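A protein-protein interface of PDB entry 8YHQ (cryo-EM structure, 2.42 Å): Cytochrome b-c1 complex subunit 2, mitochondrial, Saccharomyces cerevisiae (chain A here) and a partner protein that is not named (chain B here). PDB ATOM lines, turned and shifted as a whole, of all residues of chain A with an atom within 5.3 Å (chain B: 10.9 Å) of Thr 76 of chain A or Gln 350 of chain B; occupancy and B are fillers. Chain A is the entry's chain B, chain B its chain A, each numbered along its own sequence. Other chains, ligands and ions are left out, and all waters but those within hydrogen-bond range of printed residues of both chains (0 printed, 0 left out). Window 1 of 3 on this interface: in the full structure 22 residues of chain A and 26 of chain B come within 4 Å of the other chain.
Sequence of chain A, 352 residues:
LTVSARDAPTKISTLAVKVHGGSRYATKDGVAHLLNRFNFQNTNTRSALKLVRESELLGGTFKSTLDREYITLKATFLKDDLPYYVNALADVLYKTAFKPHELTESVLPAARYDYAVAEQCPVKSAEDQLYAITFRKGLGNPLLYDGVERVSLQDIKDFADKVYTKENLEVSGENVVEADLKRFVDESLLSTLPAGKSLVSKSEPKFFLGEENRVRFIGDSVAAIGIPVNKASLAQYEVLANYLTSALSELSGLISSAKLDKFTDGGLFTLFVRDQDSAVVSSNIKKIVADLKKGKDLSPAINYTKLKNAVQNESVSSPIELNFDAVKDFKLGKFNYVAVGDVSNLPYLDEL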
ATOM      1  N   ILE A  12       4.524 -15.300 -16.997  1.00  0.00           N
ATOM      2  CA  ILE A  12       4.441 -14.625 -18.288  1.00  0.00           C
ATOM      3  C   ILE A  12       5.023 -13.225 -18.163  1.00  0.00           C
ATOM      4  O   ILE A  12       4.763 -12.520 -17.182  1.00  0.00           O
ATOM      5  CB  ILE A  12       2.987 -14.559 -18.798  1.00  0.00           C
ATOM      6  CG1 ILE A  12       2.342 -15.946 -18.843  1.00  0.00           C
ATOM      7  CG2 ILE A  12       2.919 -13.907 -20.162  1.00  0.00           C
ATOM      8  CD1 ILE A  12       3.023 -16.953 -19.725  1.00  0.00           C
ATOM      9  N   SER A  13       5.803 -12.827 -19.165  1.00  0.00           N
ATOM     10  CA  SER A  13       6.329 -11.478 -19.296  1.00  0.00           C
ATOM     11  C   SER A  13       5.707 -10.778 -20.497  1.00  0.00           C
ATOM     12  O   SER A  13       5.106 -11.404 -21.372  1.00  0.00           O
ATOM     13  CB  SER A  13       7.849 -11.494 -19.444  1.00  0.00           C
ATOM     14  OG  SER A  13       8.486 -11.684 -18.202  1.00  0.00           O
ATOM     15  N   THR A  14       5.867  -9.458 -20.524  1.00  0.00           N
ATOM     16  CA  THR A  14       5.340  -8.613 -21.583  1.00  0.00           C
ATOM     17  C   THR A  14       6.311  -7.468 -21.823  1.00  0.00           C
ATOM     18  O   THR A  14       6.840  -6.881 -20.876  1.00  0.00           O
ATOM     19  CB  THR A  14       3.945  -8.084 -21.224  1.00  0.00           C
ATOM     20  OG1 THR A  14       2.982  -9.132 -21.381  1.00  0.00           O
ATOM     21  CG2 THR A  14       3.543  -6.934 -22.108  1.00  0.00           C
ATOM     22  N   LEU A  15       6.543  -7.166 -23.097  1.00  0.00           N
ATOM     23  CA  LEU A  15       7.471  -6.131 -23.524  1.00  0.00           C
ATOM     24  C   LEU A  15       6.804  -5.267 -24.584  1.00  0.00           C
ATOM     25  O   LEU A  15       6.120  -5.783 -25.472  1.00  0.00           O
ATOM     26  CB  LEU A  15       8.749  -6.751 -24.067  1.00  0.00           C
ATOM     27  CG  LEU A  15       9.933  -5.855 -24.388  1.00  0.00           C
ATOM     28  CD1 LEU A  15      10.535  -5.246 -23.142  1.00  0.00           C
ATOM     29  CD2 LEU A  15      10.950  -6.675 -25.124  1.00  0.00           C
ATOM     30  N   GLY A  59       7.129 -20.340 -27.422  1.00  0.00           N
ATOM     31  CA  GLY A  59       5.984 -19.847 -26.688  1.00  0.00           C
ATOM     32  C   GLY A  59       5.851 -18.338 -26.635  1.00  0.00           C
ATOM     33  O   GLY A  59       5.982 -17.742 -25.565  1.00  0.00           O
ATOM     34  N   GLY A  60       5.599 -17.706 -27.778  1.00  0.00           N
ATOM     35  CA  GLY A  60       5.381 -16.273 -27.806  1.00  0.00           C
ATOM     36  C   GLY A  60       4.670 -15.820 -29.057  1.00  0.00           C
ATOM     37  O   GLY A  60       4.634 -16.525 -30.070  1.00  0.00           O
ATOM     38  N   THR A  61       4.100 -14.618 -28.970  1.00  0.00           N
ATOM     39  CA  THR A  61       3.342 -14.005 -30.051  1.00  0.00           C
ATOM     40  C   THR A  61       3.702 -12.526 -30.145  1.00  0.00           C
ATOM     41  O   THR A  61       4.333 -11.960 -29.251  1.00  0.00           O
ATOM     42  CB  THR A  61       1.834 -14.182 -29.843  1.00  0.00           C
ATOM     43  OG1 THR A  61       1.498 -13.916 -28.478  1.00  0.00           O
ATOM     44  CG2 THR A  61       1.401 -15.595 -30.209  1.00  0.00           C
ATOM     45  N   LYS A  74       4.222  -4.812 -29.413  1.00  0.00           N
ATOM     46  CA  LYS A  74       4.098  -5.599 -28.195  1.00  0.00           C
ATOM     47  C   LYS A  74       4.458  -7.061 -28.430  1.00  0.00           C
ATOM     48  O   LYS A  74       4.146  -7.636 -29.476  1.00  0.00           O
ATOM     49  CB  LYS A  74       2.677  -5.507 -27.650  1.00  0.00           C
ATOM     50  CG  LYS A  74       2.521  -5.840 -26.197  1.00  0.00           C
ATOM     51  CD  LYS A  74       1.067  -6.040 -25.867  1.00  0.00           C
ATOM     52  CE  LYS A  74       0.837  -6.059 -24.377  1.00  0.00           C
ATOM     53  NZ  LYS A  74      -0.610  -6.130 -24.035  1.00  0.00           N
ATOM     54  N   ALA A  75       5.117  -7.654 -27.432  1.00  0.00           N
ATOM     55  CA  ALA A  75       5.410  -9.081 -27.395  1.00  0.00           C
ATOM     56  C   ALA A  75       4.989  -9.675 -26.059  1.00  0.00           C
ATOM     57  O   ALA A  75       5.125  -9.036 -25.014  1.00  0.00           O
ATOM     58  CB  ALA A  75       6.893  -9.356 -27.620  1.00  0.00           C
ATOM     59  N   THR A  76       4.481 -10.906 -26.109  1.00  0.00           N
ATOM     60  CA  THR A  76       4.076 -11.674 -24.936  1.00  0.00           C
ATOM     61  C   THR A  76       4.725 -13.049 -25.012  1.00  0.00           C
ATOM     62  O   THR A  76       4.650 -13.710 -26.051  1.00  0.00           O
ATOM     63  CB  THR A  76       2.557 -11.803 -24.868  1.00  0.00           C
ATOM     64  OG1 THR A  76       1.954 -10.551 -25.206  1.00  0.00           O
ATOM     65  CG2 THR A  76       2.114 -12.196 -23.496  1.00  0.00           C
ATOM     66  N   PHE A  77       5.356 -13.483 -23.921  1.00  0.00           N
ATOM     67  CA  PHE A  77       6.237 -14.641 -23.977  1.00  0.00           C
ATOM     68  C   PHE A  77       6.457 -15.213 -22.582  1.00  0.00           C
ATOM     69  O   PHE A  77       6.037 -14.640 -21.574  1.00  0.00           O
ATOM     70  CB  PHE A  77       7.568 -14.266 -24.634  1.00  0.00           C
ATOM     71  CG  PHE A  77       8.263 -13.098 -23.993  1.00  0.00           C
ATOM     72  CD1 PHE A  77       7.955 -11.806 -24.358  1.00  0.00           C
ATOM     73  CD2 PHE A  77       9.237 -13.293 -23.040  1.00  0.00           C
ATOM     74  CE1 PHE A  77       8.587 -10.746 -23.778  1.00  0.00           C
ATOM     75  CE2 PHE A  77       9.873 -12.234 -22.461  1.00  0.00           C
ATOM     76  CZ  PHE A  77       9.549 -10.957 -22.830  1.00  0.00           C
ATOM     77  N   LEU A  78       7.122 -16.367 -22.539  1.00  0.00           N
ATOM     78  CA  LEU A  78       7.517 -16.992 -21.284  1.00  0.00           C
ATOM     79  C   LEU A  78       8.796 -16.357 -20.751  1.00  0.00           C
ATOM     80  O   LEU A  78       9.710 -16.035 -21.513  1.00  0.00           O
ATOM     81  CB  LEU A  78       7.714 -18.495 -21.469  1.00  0.00           C
ATOM     82  CG  LEU A  78       6.540 -19.330 -21.990  1.00  0.00           C
ATOM     83  CD1 LEU A  78       6.989 -20.721 -22.328  1.00  0.00           C
ATOM     84  CD2 LEU A  78       5.405 -19.406 -21.008  1.00  0.00           C
ATOM     85  N   TYR A  85      13.333 -11.705 -27.771  1.00  0.00           N
ATOM     86  CA  TYR A  85      12.287 -10.775 -28.175  1.00  0.00           C
ATOM     87  C   TYR A  85      12.766  -9.328 -28.158  1.00  0.00           C
ATOM     88  O   TYR A  85      12.164  -8.476 -28.816  1.00  0.00           O
ATOM     89  CB  TYR A  85      11.064 -10.952 -27.276  1.00  0.00           C
ATOM     90  CG  TYR A  85      10.403 -12.295 -27.435  1.00  0.00           C
ATOM     91  CD1 TYR A  85      10.876 -13.385 -26.750  1.00  0.00           C
ATOM     92  CD2 TYR A  85       9.322 -12.475 -28.275  1.00  0.00           C
ATOM     93  CE1 TYR A  85      10.311 -14.614 -26.881  1.00  0.00           C
ATOM     94  CE2 TYR A  85       8.737 -13.712 -28.415  1.00  0.00           C
ATOM     95  CZ  TYR A  85       9.242 -14.780 -27.711  1.00  0.00           C
ATOM     96  OH  TYR A  85       8.684 -16.024 -27.826  1.00  0.00           O
ATOM     97  N   GLN B 257      -4.813 -27.666 -29.288  1.00  0.00           N
ATOM     98  CA  GLN B 257      -3.830 -26.651 -29.639  1.00  0.00           C
ATOM     99  C   GLN B 257      -3.032 -27.007 -30.888  1.00  0.00           C
ATOM    100  O   GLN B 257      -2.410 -26.122 -31.481  1.00  0.00           O
ATOM    101  CB  GLN B 257      -2.896 -26.433 -28.449  1.00  0.00           C
ATOM    102  CG  GLN B 257      -1.994 -25.227 -28.516  1.00  0.00           C
ATOM    103  CD  GLN B 257      -2.744 -23.929 -28.450  1.00  0.00           C
ATOM    104  OE1 GLN B 257      -3.621 -23.750 -27.615  1.00  0.00           O
ATOM    105  NE2 GLN B 257      -2.407 -23.013 -29.332  1.00  0.00           N
ATOM    106  N   SER B 342       4.397 -25.527 -25.894  1.00  0.00           N
ATOM    107  CA  SER B 342       4.798 -24.195 -25.471  1.00  0.00           C
ATOM    108  C   SER B 342       3.729 -23.149 -25.753  1.00  0.00           C
ATOM    109  O   SER B 342       3.684 -22.120 -25.071  1.00  0.00           O
ATOM    110  CB  SER B 342       6.115 -23.827 -26.145  1.00  0.00           C
ATOM    111  OG  SER B 342       5.981 -23.784 -27.542  1.00  0.00           O
ATOM    112  N   LEU B 343       2.866 -23.382 -26.739  1.00  0.00           N
ATOM    113  CA  LEU B 343       1.747 -22.480 -26.975  1.00  0.00           C
ATOM    114  C   LEU B 343       0.599 -22.714 -26.001  1.00  0.00           C
ATOM    115  O   LEU B 343      -0.151 -21.778 -25.707  1.00  0.00           O
ATOM    116  CB  LEU B 343       1.247 -22.624 -28.410  1.00  0.00           C
ATOM    117  CG  LEU B 343       2.065 -22.022 -29.558  1.00  0.00           C
ATOM    118  CD1 LEU B 343       1.284 -22.176 -30.830  1.00  0.00           C
ATOM    119  CD2 LEU B 343       2.455 -20.567 -29.351  1.00  0.00           C
ATOM    120  N   LEU B 344       0.428 -23.940 -25.505  1.00  0.00           N
ATOM    121  CA  LEU B 344      -0.559 -24.174 -24.458  1.00  0.00           C
ATOM    122  C   LEU B 344      -0.146 -23.494 -23.159  1.00  0.00           C
ATOM    123  O   LEU B 344      -0.994 -22.970 -22.430  1.00  0.00           O
ATOM    124  CB  LEU B 344      -0.759 -25.674 -24.244  1.00  0.00           C
ATOM    125  CG  LEU B 344      -1.705 -26.140 -23.133  1.00  0.00           C
ATOM    126  CD1 LEU B 344      -3.115 -25.707 -23.417  1.00  0.00           C
ATOM    127  CD2 LEU B 344      -1.648 -27.628 -22.971  1.00  0.00           C
ATOM    128  N   LYS B 345       1.150 -23.491 -22.856  1.00  0.00           N
ATOM    129  CA  LYS B 345       1.637 -22.820 -21.656  1.00  0.00           C
ATOM    130  C   LYS B 345       1.407 -21.317 -21.733  1.00  0.00           C
ATOM    131  O   LYS B 345       1.055 -20.683 -20.733  1.00  0.00           O
ATOM    132  CB  LYS B 345       3.121 -23.125 -21.455  1.00  0.00           C
ATOM    133  CG  LYS B 345       3.393 -24.343 -20.601  1.00  0.00           C
ATOM    134  CD  LYS B 345       4.559 -25.182 -21.085  1.00  0.00           C
ATOM    135  CE  LYS B 345       5.885 -24.543 -20.811  1.00  0.00           C
ATOM    136  NZ  LYS B 345       6.975 -25.524 -20.884  1.00  0.00           N
ATOM    137  N   LEU B 346       1.603 -20.730 -22.910  1.00  0.00           N
ATOM    138  CA  LEU B 346       1.344 -19.306 -23.090  1.00  0.00           C
ATOM    139  C   LEU B 346      -0.143 -18.996 -22.983  1.00  0.00           C
ATOM    140  O   LEU B 346      -0.525 -17.948 -22.454  1.00  0.00           O
ATOM    141  CB  LEU B 346       1.900 -18.855 -24.438  1.00  0.00           C
ATOM    142  CG  LEU B 346       1.788 -17.389 -24.844  1.00  0.00           C
ATOM    143  CD1 LEU B 346       2.651 -16.523 -23.968  1.00  0.00           C
ATOM    144  CD2 LEU B 346       2.173 -17.235 -26.294  1.00  0.00           C
ATOM    145  N   GLN B 347      -0.992 -19.890 -23.484  1.00  0.00           N
ATOM    146  CA  GLN B 347      -2.436 -19.692 -23.404  1.00  0.00           C
ATOM    147  C   GLN B 347      -2.906 -19.612 -21.955  1.00  0.00           C
ATOM    148  O   GLN B 347      -3.428 -18.580 -21.520  1.00  0.00           O
ATOM    149  CB  GLN B 347      -3.147 -20.819 -24.159  1.00  0.00           C
ATOM    150  CG  GLN B 347      -4.661 -20.857 -24.086  1.00  0.00           C
ATOM    151  CD  GLN B 347      -5.220 -22.166 -24.600  1.00  0.00           C
ATOM    152  OE1 GLN B 347      -4.551 -22.898 -25.320  1.00  0.00           O
ATOM    153  NE2 GLN B 347      -6.443 -22.478 -24.212  1.00  0.00           N
ATOM    154  N   LEU B 348      -2.754 -20.695 -21.195  1.00  0.00           N
ATOM    155  CA  LEU B 348      -3.250 -20.706 -19.826  1.00  0.00           C
ATOM    156  C   LEU B 348      -2.385 -19.893 -18.876  1.00  0.00           C
ATOM    157  O   LEU B 348      -2.824 -19.600 -17.761  1.00  0.00           O
ATOM    158  CB  LEU B 348      -3.396 -22.145 -19.306  1.00  0.00           C
ATOM    159  CG  LEU B 348      -2.232 -23.129 -19.305  1.00  0.00           C
ATOM    160  CD1 LEU B 348      -1.330 -22.965 -18.103  1.00  0.00           C
ATOM    161  CD2 LEU B 348      -2.793 -24.530 -19.352  1.00  0.00           C
ATOM    162  N   GLY B 349      -1.178 -19.512 -19.287  1.00  0.00           N
ATOM    163  CA  GLY B 349      -0.416 -18.531 -18.542  1.00  0.00           C
ATOM    164  C   GLY B 349      -0.965 -17.127 -18.620  1.00  0.00           C
ATOM    165  O   GLY B 349      -0.695 -16.322 -17.727  1.00  0.00           O
ATOM    166  N   GLN B 350      -1.721 -16.814 -19.670  1.00  0.00           N
ATOM    167  CA  GLN B 350      -2.378 -15.522 -19.799  1.00  0.00           C
ATOM    168  C   GLN B 350      -3.765 -15.506 -19.175  1.00  0.00           C
ATOM    169  O   GLN B 350      -4.252 -14.439 -18.791  1.00  0.00           O
ATOM    170  CB  GLN B 350      -2.485 -15.132 -21.273  1.00  0.00           C
ATOM    171  CG  GLN B 350      -1.216 -14.535 -21.851  1.00  0.00           C
ATOM    172  CD  GLN B 350      -1.378 -14.083 -23.281  1.00  0.00           C
ATOM    173  OE1 GLN B 350      -1.161 -12.919 -23.604  1.00  0.00           O
ATOM    174  NE2 GLN B 350      -1.761 -15.000 -24.148  1.00  0.00           N
ATOM    175  N   LEU B 351      -4.409 -16.666 -19.075  1.00  0.00           N
ATOM    176  CA  LEU B 351      -5.713 -16.767 -18.438  1.00  0.00           C
ATOM    177  C   LEU B 351      -5.606 -16.661 -16.922  1.00  0.00           C
ATOM    178  O   LEU B 351      -6.456 -16.036 -16.282  1.00  0.00           O
ATOM    179  CB  LEU B 351      -6.370 -18.084 -18.847  1.00  0.00           C
ATOM    180  CG  LEU B 351      -7.739 -18.482 -18.305  1.00  0.00           C
ATOM    181  CD1 LEU B 351      -8.846 -17.751 -19.023  1.00  0.00           C
ATOM    182  CD2 LEU B 351      -7.926 -19.967 -18.459  1.00  0.00           C
ATOM    183  N   TYR B 352      -4.571 -17.255 -16.336  1.00  0.00           N
ATOM    184  CA  TYR B 352      -4.405 -17.295 -14.891  1.00  0.00           C
ATOM    185  C   TYR B 352      -3.542 -16.163 -14.346  1.00  0.00           C
ATOM    186  O   TYR B 352      -3.423 -16.043 -13.124  1.00  0.00           O
ATOM    187  CB  TYR B 352      -3.807 -18.641 -14.476  1.00  0.00           C
ATOM    188  CG  TYR B 352      -4.801 -19.777 -14.493  1.00  0.00           C
ATOM    189  CD1 TYR B 352      -5.755 -19.906 -13.498  1.00  0.00           C
ATOM    190  CD2 TYR B 352      -4.789 -20.715 -15.507  1.00  0.00           C
ATOM    191  CE1 TYR B 352      -6.666 -20.937 -13.519  1.00  0.00           C
ATOM    192  CE2 TYR B 352      -5.689 -21.743 -15.536  1.00  0.00           C
ATOM    193  CZ  TYR B 352      -6.629 -21.853 -14.541  1.00  0.00           C
ATOM    194  OH  TYR B 352      -7.534 -22.885 -14.566  1.00  0.00           O
ATOM    195  N   GLU B 353      -2.946 -15.338 -15.206  1.00  0.00           N
ATOM    196  CA  GLU B 353      -2.117 -14.214 -14.777  1.00  0.00           C
ATOM    197  C   GLU B 353      -2.484 -12.954 -15.548  1.00  0.00           C
ATOM    198  O   GLU B 353      -1.622 -12.213 -16.022  1.00  0.00           O
ATOM    199  CB  GLU B 353      -0.635 -14.523 -14.946  1.00  0.00           C
ATOM    200  CG  GLU B 353      -0.137 -15.664 -14.090  1.00  0.00           C
ATOM    201  CD  GLU B 353       1.313 -15.987 -14.350  1.00  0.00           C
ATOM    202  OE1 GLU B 353       1.866 -15.480 -15.347  1.00  0.00           O
ATOM    203  OE2 GLU B 353       1.904 -16.744 -13.554  1.00  0.00           O
ATOM    204  N   SER B 354      -3.778 -12.698 -15.688  1.00  0.00           N
ATOM    205  CA  SER B 354      -4.243 -11.393 -16.134  1.00  0.00           C
ATOM    206  C   SER B 354      -4.189 -10.436 -14.945  1.00  0.00           C
ATOM    207  O   SER B 354      -3.802 -10.810 -13.834  1.00  0.00           O
ATOM    208  CB  SER B 354      -5.641 -11.494 -16.733  1.00  0.00           C
ATOM    209  OG  SER B 354      -6.540 -12.131 -15.852  1.00  0.00           O
ATOM    210  N   GLY B 355      -4.585  -9.189 -15.168  1.00  0.00           N
ATOM    211  CA  GLY B 355      -4.547  -8.176 -14.131  1.00  0.00           C
ATOM    212  C   GLY B 355      -5.867  -7.914 -13.437  1.00  0.00           C
ATOM    213  O   GLY B 355      -5.920  -7.095 -12.519  1.00  0.00           O
ATOM    214  N   ASN B 356      -6.932  -8.595 -13.856  1.00  0.00           N
ATOM    215  CA  ASN B 356      -8.267  -8.339 -13.331  1.00  0.00           C
ATOM    216  C   ASN B 356      -8.538  -9.254 -12.141  1.00  0.00           C
ATOM    217  O   ASN B 356      -8.557 -10.478 -12.317  1.00  0.00           O
ATOM    218  CB  ASN B 356      -9.310  -8.569 -14.409  1.00  0.00           C
ATOM    219  CG  ASN B 356     -10.597  -7.807 -14.161  1.00  0.00           C
ATOM    220  OD1 ASN B 356     -10.709  -7.018 -13.223  1.00  0.00           O
ATOM    221  ND2 ASN B 356     -11.586  -8.045 -15.010  1.00  0.00           N
ATOM    222  N   PRO B 357      -8.747  -8.730 -10.925  1.00  0.00           N
ATOM    223  CA  PRO B 357      -9.062  -9.626  -9.803  1.00  0.00           C
ATOM    224  C   PRO B 357     -10.432 -10.275  -9.891  1.00  0.00           C
ATOM    225  O   PRO B 357     -10.674 -11.257  -9.179  1.00  0.00           O
ATOM    226  CB  PRO B 357      -8.958  -8.707  -8.578  1.00  0.00           C
ATOM    227  CG  PRO B 357      -8.158  -7.584  -9.013  1.00  0.00           C
ATOM    228  CD  PRO B 357      -8.503  -7.365 -10.432  1.00  0.00           C
ATOM    229  N   ASN B 359     -11.665 -11.848 -12.559  1.00  0.00           N
ATOM    230  CA  ASN B 359     -11.466 -13.130 -13.226  1.00  0.00           C
ATOM    231  C   ASN B 359     -10.792 -14.129 -12.300  1.00  0.00           C
ATOM    232  O   ASN B 359     -11.089 -15.329 -12.344  1.00  0.00           O
ATOM    233  CB  ASN B 359     -10.637 -12.940 -14.493  1.00  0.00           C
ATOM    234  CG  ASN B 359     -11.401 -12.247 -15.595  1.00  0.00           C
ATOM    235  OD1 ASN B 359     -12.630 -12.279 -15.638  1.00  0.00           O
ATOM    236  ND2 ASN B 359     -10.673 -11.615 -16.500  1.00  0.00           N
ATOM    237  N   ASP B 360      -9.868 -13.652 -11.467  1.00  0.00           N
ATOM    238  CA  ASP B 360      -9.213 -14.508 -10.487  1.00  0.00           C
ATOM    239  C   ASP B 360     -10.221 -15.144  -9.539  1.00  0.00           C
ATOM    240  O   ASP B 360     -10.119 -16.333  -9.221  1.00  0.00           O
ATOM    241  CB  ASP B 360      -8.197 -13.685  -9.705  1.00  0.00           C
ATOM    242  CG  ASP B 360      -6.985 -13.310 -10.531  1.00  0.00           C
ATOM    243  OD1 ASP B 360      -6.944 -13.650 -11.730  1.00  0.00           O
ATOM    244  OD2 ASP B 360      -6.068 -12.667  -9.978  1.00  0.00           O
ATOM    245  N   LEU B 363     -12.304 -17.984 -11.217  1.00  0.00           N
ATOM    246  CA  LEU B 363     -11.485 -19.173 -11.436  1.00  0.00           C
ATOM    247  C   LEU B 363     -11.202 -19.899 -10.127  1.00  0.00           C
ATOM    248  O   LEU B 363     -11.294 -21.129 -10.052  1.00  0.00           O
ATOM    249  CB  LEU B 363     -10.173 -18.790 -12.121  1.00  0.00           C
ATOM    250  CG  LEU B 363     -10.206 -18.358 -13.585  1.00  0.00           C
ATOM    251  CD1 LEU B 363      -8.862 -17.794 -13.975  1.00  0.00           C
ATOM    252  CD2 LEU B 363     -10.577 -19.501 -14.496  1.00  0.00           C
ATOM    253  N   LEU B 377       0.271 -23.010 -11.060  1.00  0.00           N
ATOM    254  CA  LEU B 377       0.695 -22.951 -12.448  1.00  0.00           C
ATOM    255  C   LEU B 377       2.063 -23.576 -12.672  1.00  0.00           C
ATOM    256  O   LEU B 377       2.347 -24.024 -13.786  1.00  0.00           O
ATOM    257  CB  LEU B 377       0.696 -21.496 -12.912  1.00  0.00           C
ATOM    258  CG  LEU B 377       0.718 -21.221 -14.411  1.00  0.00           C
ATOM    259  CD1 LEU B 377      -0.540 -21.724 -15.084  1.00  0.00           C
ATOM    260  CD2 LEU B 377       0.885 -19.746 -14.667  1.00  0.00           C
ATOM    261  N   PHE B 381       2.518 -26.874 -15.516  1.00  0.00           N
ATOM    262  CA  PHE B 381       3.522 -26.858 -16.573  1.00  0.00           C
ATOM    263  C   PHE B 381       4.297 -28.167 -16.614  1.00  0.00           C
ATOM    264  O   PHE B 381       4.605 -28.676 -17.697  1.00  0.00           O
ATOM    265  CB  PHE B 381       4.478 -25.682 -16.366  1.00  0.00           C
ATOM    266  CG  PHE B 381       3.962 -24.349 -16.858  1.00  0.00           C
ATOM    267  CD1 PHE B 381       2.610 -24.088 -16.995  1.00  0.00           C
ATOM    268  CD2 PHE B 381       4.853 -23.345 -17.169  1.00  0.00           C
ATOM    269  CE1 PHE B 381       2.174 -22.863 -17.442  1.00  0.00           C
ATOM    270  CE2 PHE B 381       4.412 -22.124 -17.612  1.00  0.00           C
ATOM    271  CZ  PHE B 381       3.077 -21.885 -17.747  1.00  0.00           C
ATOM    272  N   ILE B 384       2.510 -30.846 -18.430  1.00  0.00           N
ATOM    273  CA  ILE B 384       2.419 -30.645 -19.871  1.00  0.00           C
ATOM    274  C   ILE B 384       3.719 -31.048 -20.549  1.00  0.00           C
ATOM    275  O   ILE B 384       3.705 -31.600 -21.654  1.00  0.00           O
ATOM    276  CB  ILE B 384       2.042 -29.182 -20.180  1.00  0.00           C
ATOM    277  CG1 ILE B 384       0.600 -28.909 -19.772  1.00  0.00           C
ATOM    278  CG2 ILE B 384       2.204 -28.874 -21.650  1.00  0.00           C
ATOM    279  CD1 ILE B 384       0.268 -27.465 -19.573  1.00  0.00           C
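Of the 23 printed residues of chain B, 5 touch a printed residue of chain A.
Printed residues of chain B that touch a printed residue of chain A: Ser 342, Leu 346, Gly 349, Gln 350 and Glu 353.
Hydrophobic or aromatic side chains of chain B that line the printed part of chain A: Leu 346.
Of the 13 printed residues of chain A, 4 touch a printed residue of chain B.
Hydrophobic or aromatic side chains of chain A within 4 Å of the printed part of chain B: Ile 12.
Along chain A the printed residues that touch a printed residue of chain B span positions 12 to 76.
Among the printed residues, 6 pairs touch across the chains.
Among the printed residues, no Asp or Glu carboxylate lies within 4 Å of a Lys or Arg side-chain nitrogen of the other chain.
OE1 of Glu 353 of chain B sits at hydrogen-bond distance from N of Ile 12 of chain A, 3.1 Å away.
N of Thr 61 of chain A sits at hydrogen-bond distance from O of Thr 76 of chain A, 3.1 Å away.
Ile 12 of chain A touches Gly 349 of chain B (CG1 to O, 3.3 Å).
Gly 59 of chain A touches Ser 342 of chain B (CA to O, 3.6 Å).
Leu 346 of chain B touches Gly 59 of chain A (CD2 to C, 3.9 Å).
Gly 60 of chain A touches Leu 346 of chain B (CA to CD2, 3.7 Å).
CG2 of Thr 76 of chain A touches OE1 of Gln 350 of chain B, at 3.4 Å.
Thr 76 of chain A touches just one residue of chain B: Gln 350 (3.4 Å).
Gln 350 of chain B touches one residue of chain A.
Gly 60 of chain A touches just one residue of chain B: Leu 346.
Thr 61 of chain A touches none of the printed residues of chain B.
No residue of chain B comes within 4 Å of Ala 75 of chain A.
No residue of chain B comes within 4 Å of Phe 77 of chain A.
Of the printed residues of chain B, Ile 12 of chain A touches Gly 349 and Glu 353.
Printed residues of chain A within 4 Å of Glu 353 of chain B: Ile 12 (3.1 Å).
Printed residues of chain A within 4 Å of Ser 342 of chain B: Gly 59.
Of the printed residues of chain B, Gly 59 of chain A touches Ser 342 (3.6 Å) and Leu 346 (3.9 Å).
Leu 78 of chain A touches none of the printed residues of chain B.
Asp 360 of chain B touches none of the printed residues of chain A.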
